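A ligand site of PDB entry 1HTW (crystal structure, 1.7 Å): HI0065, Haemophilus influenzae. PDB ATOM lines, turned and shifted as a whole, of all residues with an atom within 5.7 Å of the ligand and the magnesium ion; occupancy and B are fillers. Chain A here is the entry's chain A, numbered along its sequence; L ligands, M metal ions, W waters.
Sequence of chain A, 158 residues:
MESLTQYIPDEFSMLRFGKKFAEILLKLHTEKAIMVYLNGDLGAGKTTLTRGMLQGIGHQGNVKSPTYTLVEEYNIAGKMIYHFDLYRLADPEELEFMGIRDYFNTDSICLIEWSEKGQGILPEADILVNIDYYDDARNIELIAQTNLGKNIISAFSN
Water W4 bridges the side-chain carboxylate (OD2) of Asp 85 (2.6 Å) and the side-chain hydroxyl (OG) of Ser 65 (2.6 Å).
Water W10 bridges the backbone NH of Glu 11 and a nitrogen (N2) of the ligand.
Water W3 bridges the backbone carbonyl oxygen (O) of Gly 43 and an oxygen (O8) of the ligand.
Water W5 lies within hydrogen-bond range of NH2 of Arg 138 (2.8 Å), OD1 of Asp 136 (3.0 Å) and O of Asp 135 (3.1 Å).
Within 4 Å of the magnesium ion: Thr 47 and Glu 113.
The nearest printed residue that does not touch the magnesium ion is Asp 85 (4.4 Å).
An oxygen (O1) of the ligand lies close to the backbone NH (N) of Thr 47 (2.9 Å).
The side-chain carboxylate of Glu 11 is in hydrogen-bond range of an oxygen (O10) of the ligand (2.5 Å).
N of Lys 46 is in hydrogen-bond range of O2 of the ligand (2.8 Å).
The side-chain amino group (NZ) of Lys 46 lies within salt-bridge range of an oxygen (O2) of the ligand (2.6 Å).
An oxygen (O5) of the ligand is in hydrogen-bond range of the backbone NH of Thr 48 (2.8 Å).
The side-chain hydroxyl (OG1) of Thr 48 sits at hydrogen-bond distance from an oxygen (O5) of the ligand.
The backbone NH of Gly 43 sits at hydrogen-bond distance from an oxygen (O3) of the ligand, at 2.9 Å.
N3 of the ligand sits at hydrogen-bond distance from O of Asp 136 (2.9 Å).
An oxygen (O2) of the ligand is in hydrogen-bond range of the backbone NH (N) of Gly 45 (3.0 Å).
The backbone carbonyl oxygen of Asp 10 sits close to a nitrogen (N3) of the ligand (3.3 Å).
The guanidinium group (NH2) of Arg 138 lies within hydrogen-bond range of an oxygen (O8) of the ligand (3.3 Å).
N of Ala 44 sits at hydrogen-bond distance from O2 of the ligand (3.4 Å).
Met 14 touches the ligand.
Asp 41 touches the ligand.
Leu 42 touches the ligand.
Hydrophobic or aromatic side chains within 4 Å of the ligand: Met 14 and Leu 42.
Of the 23 residues printed, 14 come within 4 Å of the ligand.
The magnesium ion is bound by O1 of the ligand.
OG1 of Thr 47 is bound to the magnesium ion.
Water W8 binds the magnesium ion (2.1 Å).
The magnesium ion is bound by OE1 of Glu 113, 2.2 Å away.
Water W7 binds the magnesium ion, at 2.2 Å.
Water W4 binds the magnesium ion, at 2.3 Å.
The magnesium ion has six donor atoms within binding distance.
NE2 of His 83 sits at hydrogen-bond distance from OE2 of Glu 113 (2.8 Å).
O of Asp 41 is in hydrogen-bond range of NZ of Lys 46 (3.1 Å).
The side-chain amino group of Lys 46 lies close to the backbone carbonyl oxygen of Gly 40 (3.1 Å).
The backbone carbonyl oxygen (O) of Gly 43 is in hydrogen-bond range of the guanidinium group (NH2) of Arg 138, at 3.3 Å.
The guanidinium group of Arg 138 is in hydrogen-bond range of the backbone carbonyl oxygen of Ala 44.
N of Arg 138 sits at hydrogen-bond distance from O of Ile 8 (2.8 Å).
The backbone carbonyl oxygen (O) of Asp 135 lies within hydrogen-bond range of the guanidinium group (NH1) of Arg 138 (2.9 Å).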
ATOM      1  N   ILE A   8      17.073  33.638 -12.582  1.00  0.00           N
ATOM      2  CA  ILE A   8      17.695  32.527 -13.382  1.00  0.00           C
ATOM      3  C   ILE A   8      16.519  31.662 -13.931  1.00  0.00           C
ATOM      4  O   ILE A   8      16.015  30.803 -13.216  1.00  0.00           O
ATOM      5  CB  ILE A   8      18.467  31.674 -12.371  1.00  0.00           C
ATOM      6  CG1 ILE A   8      19.603  32.494 -11.733  1.00  0.00           C
ATOM      7  CG2 ILE A   8      19.042  30.467 -13.162  1.00  0.00           C
ATOM      8  CD1 ILE A   8      20.642  33.079 -12.708  1.00  0.00           C
ATOM      9  N   PRO A   9      16.110  31.997 -15.128  1.00  0.00           N
ATOM     10  CA  PRO A   9      14.866  31.392 -15.675  1.00  0.00           C
ATOM     11  C   PRO A   9      14.900  29.925 -15.947  1.00  0.00           C
ATOM     12  O   PRO A   9      13.874  29.223 -15.998  1.00  0.00           O
ATOM     13  CB  PRO A   9      14.617  32.201 -16.938  1.00  0.00           C
ATOM     14  CG  PRO A   9      15.838  32.907 -17.266  1.00  0.00           C
ATOM     15  CD  PRO A   9      16.619  33.065 -15.975  1.00  0.00           C
ATOM     16  N   ASP A  10      16.098  29.313 -16.123  1.00  0.00           N
ATOM     17  CA  ASP A  10      16.188  27.904 -16.454  1.00  0.00           C
ATOM     18  C   ASP A  10      17.613  27.416 -16.209  1.00  0.00           C
ATOM     19  O   ASP A  10      18.459  28.226 -15.757  1.00  0.00           O
ATOM     20  CB  ASP A  10      15.881  27.765 -17.970  1.00  0.00           C
ATOM     21  CG  ASP A  10      16.576  28.804 -18.803  1.00  0.00           C
ATOM     22  OD1 ASP A  10      17.820  28.989 -18.712  1.00  0.00           O
ATOM     23  OD2 ASP A  10      15.894  29.515 -19.587  1.00  0.00           O
ATOM     24  N   GLU A  11      17.779  26.101 -16.314  1.00  0.00           N
ATOM     25  CA  GLU A  11      19.098  25.545 -15.994  1.00  0.00           C
ATOM     26  C   GLU A  11      20.214  26.086 -16.844  1.00  0.00           C
ATOM     27  O   GLU A  11      21.316  26.277 -16.245  1.00  0.00           O
ATOM     28  CB  GLU A  11      18.984  24.009 -16.036  1.00  0.00           C
ATOM     29  CG  GLU A  11      20.297  23.371 -15.574  1.00  0.00           C
ATOM     30  CD  GLU A  11      20.157  21.901 -15.276  1.00  0.00           C
ATOM     31  OE1 GLU A  11      19.032  21.456 -14.967  1.00  0.00           O
ATOM     32  OE2 GLU A  11      21.187  21.188 -15.371  1.00  0.00           O
ATOM     33  N   MET A  14      21.488  29.068 -15.239  1.00  0.00           N
ATOM     34  CA  MET A  14      22.200  28.859 -14.002  1.00  0.00           C
ATOM     35  C   MET A  14      23.705  28.577 -14.370  1.00  0.00           C
ATOM     36  O   MET A  14      24.568  29.028 -13.645  1.00  0.00           O
ATOM     37  CB  MET A  14      21.716  27.640 -13.223  1.00  0.00           C
ATOM     38  CG  MET A  14      22.357  27.430 -11.886  1.00  0.00           C
ATOM     39  SD  MET A  14      22.129  28.854 -10.617  1.00  0.00           S
ATOM     40  CE  MET A  14      20.814  28.104  -9.508  1.00  0.00           C
ATOM     41  N   GLY A  40      20.621  27.152   0.253  1.00  0.00           N
ATOM     42  CA  GLY A  40      19.380  26.849  -0.498  1.00  0.00           C
ATOM     43  C   GLY A  40      18.956  25.422  -0.134  1.00  0.00           C
ATOM     44  O   GLY A  40      19.669  24.661   0.488  1.00  0.00           O
ATOM     45  N   ASP A  41      17.605  25.231  -0.230  1.00  0.00           N
ATOM     46  CA  ASP A  41      17.117  23.903   0.139  1.00  0.00           C
ATOM     47  C   ASP A  41      17.640  22.808  -0.761  1.00  0.00           C
ATOM     48  O   ASP A  41      18.130  23.014  -1.863  1.00  0.00           O
ATOM     49  CB  ASP A  41      15.560  23.936  -0.118  1.00  0.00           C
ATOM     50  CG  ASP A  41      14.861  24.760   0.924  1.00  0.00           C
ATOM     51  OD1 ASP A  41      15.415  25.153   1.957  1.00  0.00           O
ATOM     52  OD2 ASP A  41      13.623  25.014   0.681  1.00  0.00           O
ATOM     53  N   LEU A  42      17.468  21.563  -0.285  1.00  0.00           N
ATOM     54  CA  LEU A  42      17.792  20.425  -1.183  1.00  0.00           C
ATOM     55  C   LEU A  42      17.102  20.566  -2.493  1.00  0.00           C
ATOM     56  O   LEU A  42      15.864  20.776  -2.608  1.00  0.00           O
ATOM     57  CB  LEU A  42      17.422  19.143  -0.409  1.00  0.00           C
ATOM     58  CG  LEU A  42      17.878  17.831  -1.011  1.00  0.00           C
ATOM     59  CD1 LEU A  42      19.391  17.663  -0.869  1.00  0.00           C
ATOM     60  CD2 LEU A  42      17.145  16.675  -0.330  1.00  0.00           C
ATOM     61  N   GLY A  43      17.834  20.514  -3.597  1.00  0.00           N
ATOM     62  CA  GLY A  43      17.336  20.647  -4.955  1.00  0.00           C
ATOM     63  C   GLY A  43      17.270  22.053  -5.529  1.00  0.00           C
ATOM     64  O   GLY A  43      16.861  22.228  -6.672  1.00  0.00           O
ATOM     65  N   ALA A  44      17.660  23.068  -4.747  1.00  0.00           N
ATOM     66  CA  ALA A  44      17.649  24.451  -5.166  1.00  0.00           C
ATOM     67  C   ALA A  44      18.603  24.727  -6.335  1.00  0.00           C
ATOM     68  O   ALA A  44      18.391  25.591  -7.133  1.00  0.00           O
ATOM     69  CB  ALA A  44      17.976  25.382  -4.011  1.00  0.00           C
ATOM     70  N   GLY A  45      19.727  23.915  -6.381  1.00  0.00           N
ATOM     71  CA  GLY A  45      20.628  24.087  -7.534  1.00  0.00           C
ATOM     72  C   GLY A  45      22.075  24.426  -7.023  1.00  0.00           C
ATOM     73  O   GLY A  45      22.773  24.982  -7.906  1.00  0.00           O
ATOM     74  N   LYS A  46      22.411  24.156  -5.816  1.00  0.00           N
ATOM     75  CA  LYS A  46      23.768  24.553  -5.296  1.00  0.00           C
ATOM     76  C   LYS A  46      24.831  23.785  -6.077  1.00  0.00           C
ATOM     77  O   LYS A  46      25.777  24.376  -6.639  1.00  0.00           O
ATOM     78  CB  LYS A  46      23.929  24.298  -3.810  1.00  0.00           C
ATOM     79  CG  LYS A  46      22.947  24.957  -2.851  1.00  0.00           C
ATOM     80  CD  LYS A  46      23.066  24.552  -1.406  1.00  0.00           C
ATOM     81  CE  LYS A  46      22.674  23.109  -1.107  1.00  0.00           C
ATOM     82  NZ  LYS A  46      21.210  22.833  -1.429  1.00  0.00           N
ATOM     83  N   THR A  47      24.648  22.474  -6.212  1.00  0.00           N
ATOM     84  CA  THR A  47      25.551  21.653  -7.042  1.00  0.00           C
ATOM     85  C   THR A  47      25.505  21.936  -8.474  1.00  0.00           C
ATOM     86  O   THR A  47      26.555  21.928  -9.206  1.00  0.00           O
ATOM     87  CB  THR A  47      25.332  20.172  -6.637  1.00  0.00           C
ATOM     88  OG1 THR A  47      25.642  19.997  -5.289  1.00  0.00           O
ATOM     89  CG2 THR A  47      26.232  19.289  -7.530  1.00  0.00           C
ATOM     90  N   THR A  48      24.362  22.305  -9.112  1.00  0.00           N
ATOM     91  CA  THR A  48      24.314  22.689 -10.502  1.00  0.00           C
ATOM     92  C   THR A  48      25.046  24.044 -10.773  1.00  0.00           C
ATOM     93  O   THR A  48      25.713  24.132 -11.784  1.00  0.00           O
ATOM     94  CB  THR A  48      22.854  22.911 -10.984  1.00  0.00           C
ATOM     95  OG1 THR A  48      22.306  21.528 -10.880  1.00  0.00           O
ATOM     96  CG2 THR A  48      22.768  23.360 -12.396  1.00  0.00           C
ATOM     97  N   LEU A  49      24.906  24.919  -9.784  1.00  0.00           N
ATOM     98  CA  LEU A  49      25.672  26.209  -9.948  1.00  0.00           C
ATOM     99  C   LEU A  49      27.200  25.903  -9.826  1.00  0.00           C
ATOM    100  O   LEU A  49      27.860  26.448 -10.719  1.00  0.00           O
ATOM    101  CB  LEU A  49      25.318  27.122  -8.754  1.00  0.00           C
ATOM    102  CG  LEU A  49      26.170  28.404  -8.675  1.00  0.00           C
ATOM    103  CD1 LEU A  49      26.174  29.162  -9.977  1.00  0.00           C
ATOM    104  CD2 LEU A  49      25.669  29.309  -7.526  1.00  0.00           C
ATOM    105  N   SER A  65      28.970  15.560  -6.409  1.00  0.00           N
ATOM    106  CA  SER A  65      29.023  16.084  -5.048  1.00  0.00           C
ATOM    107  C   SER A  65      29.693  15.073  -4.105  1.00  0.00           C
ATOM    108  O   SER A  65      29.368  13.875  -4.124  1.00  0.00           O
ATOM    109  CB  SER A  65      27.545  16.265  -4.582  1.00  0.00           C
ATOM    110  OG  SER A  65      27.465  16.487  -3.206  1.00  0.00           O
ATOM    111  N   HIS A  83      35.430  21.898  -3.690  1.00  0.00           N
ATOM    112  CA  HIS A  83      33.933  21.864  -3.555  1.00  0.00           C
ATOM    113  C   HIS A  83      33.672  21.050  -2.305  1.00  0.00           C
ATOM    114  O   HIS A  83      34.119  19.903  -2.119  1.00  0.00           O
ATOM    115  CB  HIS A  83      33.372  21.160  -4.802  1.00  0.00           C
ATOM    116  CG  HIS A  83      31.863  21.013  -4.737  1.00  0.00           C
ATOM    117  ND1 HIS A  83      31.218  20.051  -5.466  1.00  0.00           N
ATOM    118  CD2 HIS A  83      30.943  21.745  -4.084  1.00  0.00           C
ATOM    119  CE1 HIS A  83      29.898  20.149  -5.235  1.00  0.00           C
ATOM    120  NE2 HIS A  83      29.684  21.197  -4.432  1.00  0.00           N
ATOM    121  N   ASP A  85      30.707  19.550   0.411  1.00  0.00           N
ATOM    122  CA  ASP A  85      29.297  19.327   0.817  1.00  0.00           C
ATOM    123  C   ASP A  85      29.401  18.755   2.242  1.00  0.00           C
ATOM    124  O   ASP A  85      29.879  17.619   2.379  1.00  0.00           O
ATOM    125  CB  ASP A  85      28.534  18.329  -0.043  1.00  0.00           C
ATOM    126  CG  ASP A  85      27.057  18.292   0.498  1.00  0.00           C
ATOM    127  OD1 ASP A  85      26.910  18.648   1.673  1.00  0.00           O
ATOM    128  OD2 ASP A  85      26.175  17.993  -0.280  1.00  0.00           O
ATOM    129  N   GLU A 113      28.768  23.808   0.370  1.00  0.00           N
ATOM    130  CA  GLU A 113      27.350  23.495   0.622  1.00  0.00           C
ATOM    131  C   GLU A 113      27.223  23.030   2.045  1.00  0.00           C
ATOM    132  O   GLU A 113      28.147  22.444   2.638  1.00  0.00           O
ATOM    133  CB  GLU A 113      26.850  22.406  -0.343  1.00  0.00           C
ATOM    134  CG  GLU A 113      26.818  22.864  -1.785  1.00  0.00           C
ATOM    135  CD  GLU A 113      26.330  21.880  -2.793  1.00  0.00           C
ATOM    136  OE1 GLU A 113      25.216  21.297  -2.577  1.00  0.00           O
ATOM    137  OE2 GLU A 113      26.955  21.715  -3.850  1.00  0.00           O
ATOM    138  N   ASP A 135       9.442  25.784  -9.505  1.00  0.00           N
ATOM    139  CA  ASP A 135       9.406  24.997 -10.738  1.00  0.00           C
ATOM    140  C   ASP A 135      10.854  24.870 -11.258  1.00  0.00           C
ATOM    141  O   ASP A 135      11.694  24.519 -10.409  1.00  0.00           O
ATOM    142  CB  ASP A 135       8.457  25.602 -11.762  1.00  0.00           C
ATOM    143  CG  ASP A 135       6.993  25.410 -11.397  1.00  0.00           C
ATOM    144  OD1 ASP A 135       6.707  24.466 -10.627  1.00  0.00           O
ATOM    145  OD2 ASP A 135       6.124  26.140 -11.933  1.00  0.00           O
ATOM    146  N   ASP A 136      11.135  25.175 -12.480  1.00  0.00           N
ATOM    147  CA  ASP A 136      12.500  25.037 -13.002  1.00  0.00           C
ATOM    148  C   ASP A 136      13.190  26.414 -13.080  1.00  0.00           C
ATOM    149  O   ASP A 136      14.185  26.558 -13.799  1.00  0.00           O
ATOM    150  CB  ASP A 136      12.493  24.382 -14.374  1.00  0.00           C
ATOM    151  CG  ASP A 136      12.189  22.892 -14.295  1.00  0.00           C
ATOM    152  OD1 ASP A 136      12.240  22.311 -13.192  1.00  0.00           O
ATOM    153  OD2 ASP A 136      11.868  22.316 -15.365  1.00  0.00           O
ATOM    154  N   ALA A 137      12.593  27.408 -12.411  1.00  0.00           N
ATOM    155  CA  ALA A 137      13.247  28.726 -12.362  1.00  0.00           C
ATOM    156  C   ALA A 137      13.838  28.931 -10.987  1.00  0.00           C
ATOM    157  O   ALA A 137      13.465  28.315  -9.996  1.00  0.00           O
ATOM    158  CB  ALA A 137      12.351  29.880 -12.749  1.00  0.00           C
ATOM    159  N   ARG A 138      14.797  29.857 -10.884  1.00  0.00           N
ATOM    160  CA  ARG A 138      15.441  30.190  -9.643  1.00  0.00           C
ATOM    161  C   ARG A 138      15.640  31.695  -9.543  1.00  0.00           C
ATOM    162  O   ARG A 138      15.551  32.421 -10.506  1.00  0.00           O
ATOM    163  CB  ARG A 138      16.863  29.497  -9.520  1.00  0.00           C
ATOM    164  CG  ARG A 138      16.833  27.987  -9.685  1.00  0.00           C
ATOM    165  CD  ARG A 138      16.239  27.208  -8.582  1.00  0.00           C
ATOM    166  NE  ARG A 138      16.354  25.738  -8.728  1.00  0.00           N
ATOM    167  CZ  ARG A 138      15.421  24.998  -9.309  1.00  0.00           C
ATOM    168  NH1 ARG A 138      14.286  25.549  -9.758  1.00  0.00           N
ATOM    169  NH2 ARG A 138      15.516  23.660  -9.341  1.00  0.00           N
HETATM  170  P1  LIG L   1      21.306  21.164  -4.552  1.00  0.00           P
HETATM  171  O1  LIG L   1      22.823  20.937  -4.594  1.00  0.00           O
HETATM  172  O2  LIG L   1      20.947  22.491  -4.033  1.00  0.00           O
HETATM  173  O3  LIG L   1      20.690  19.986  -3.680  1.00  0.00           O
HETATM  174  P2  LIG L   1      21.243  20.195  -7.281  1.00  0.00           P
HETATM  175  O4  LIG L   1      21.840  18.863  -7.005  1.00  0.00           O
HETATM  176  O5  LIG L   1      22.042  21.095  -8.131  1.00  0.00           O
HETATM  177  O6  LIG L   1      20.750  20.905  -5.958  1.00  0.00           O
HETATM  178  O7  LIG L   1      19.850  19.915  -8.032  1.00  0.00           O
HETATM  179  C1  LIG L   1      19.160  20.849  -8.814  1.00  0.00           C
HETATM  180  C2  LIG L   1      18.124  20.057  -9.674  1.00  0.00           C
HETATM  181  O8  LIG L   1      17.185  20.980 -10.226  1.00  0.00           O
HETATM  182  C3  LIG L   1      18.756  19.301 -10.815  1.00  0.00           C
HETATM  183  O9  LIG L   1      18.119  17.986 -10.962  1.00  0.00           O
HETATM  184  C4  LIG L   1      18.543  20.266 -11.959  1.00  0.00           C
HETATM  185  O10 LIG L   1      18.603  19.672 -13.246  1.00  0.00           O
HETATM  186  C5  LIG L   1      17.194  20.923 -11.600  1.00  0.00           C
HETATM  187  N1  LIG L   1      17.050  22.251 -12.136  1.00  0.00           N
HETATM  188  C6  LIG L   1      15.994  22.734 -12.852  1.00  0.00           C
HETATM  189  N2  LIG L   1      16.007  23.993 -13.163  1.00  0.00           N
HETATM  190  C7  LIG L   1      17.154  24.396 -12.641  1.00  0.00           C
HETATM  191  C8  LIG L   1      17.637  25.684 -12.623  1.00  0.00           C
HETATM  192  N3  LIG L   1      17.028  26.745 -13.133  1.00  0.00           N
HETATM  193  N4  LIG L   1      18.778  25.844 -11.907  1.00  0.00           N
HETATM  194  C9  LIG L   1      19.363  24.798 -11.309  1.00  0.00           C
HETATM  195  N5  LIG L   1      18.949  23.515 -11.217  1.00  0.00           N
HETATM  196  C10 LIG L   1      17.821  23.406 -11.976  1.00  0.00           C
HETATM  197 MG    MG M   1      24.230  19.773  -3.768  1.00  0.00          MG
HETATM  198  O   HOH W   1      19.934  16.847 -13.460  1.00  0.00           O
HETATM  199  O   HOH W   2      14.129  19.738 -10.356  1.00  0.00           O
HETATM  200  O   HOH W   3      15.196  20.107  -7.728  1.00  0.00           O
HETATM  201  O   HOH W   4      25.606  18.253  -2.790  1.00  0.00           O
HETATM  202  O   HOH W   5      13.578  22.093 -10.521  1.00  0.00           O
HETATM  203  O   HOH W   6      23.287  17.740  -8.939  1.00  0.00           O
HETATM  204  O   HOH W   7      23.438  18.032  -4.850  1.00  0.00           O
HETATM  205  O   HOH W   8      22.829  19.438  -2.199  1.00  0.00           O
HETATM  206  O   HOH W   9      19.831  17.702  -4.653  1.00  0.00           O
HETATM  207  O   HOH W  10      15.605  24.475 -16.413  1.00  0.00           O
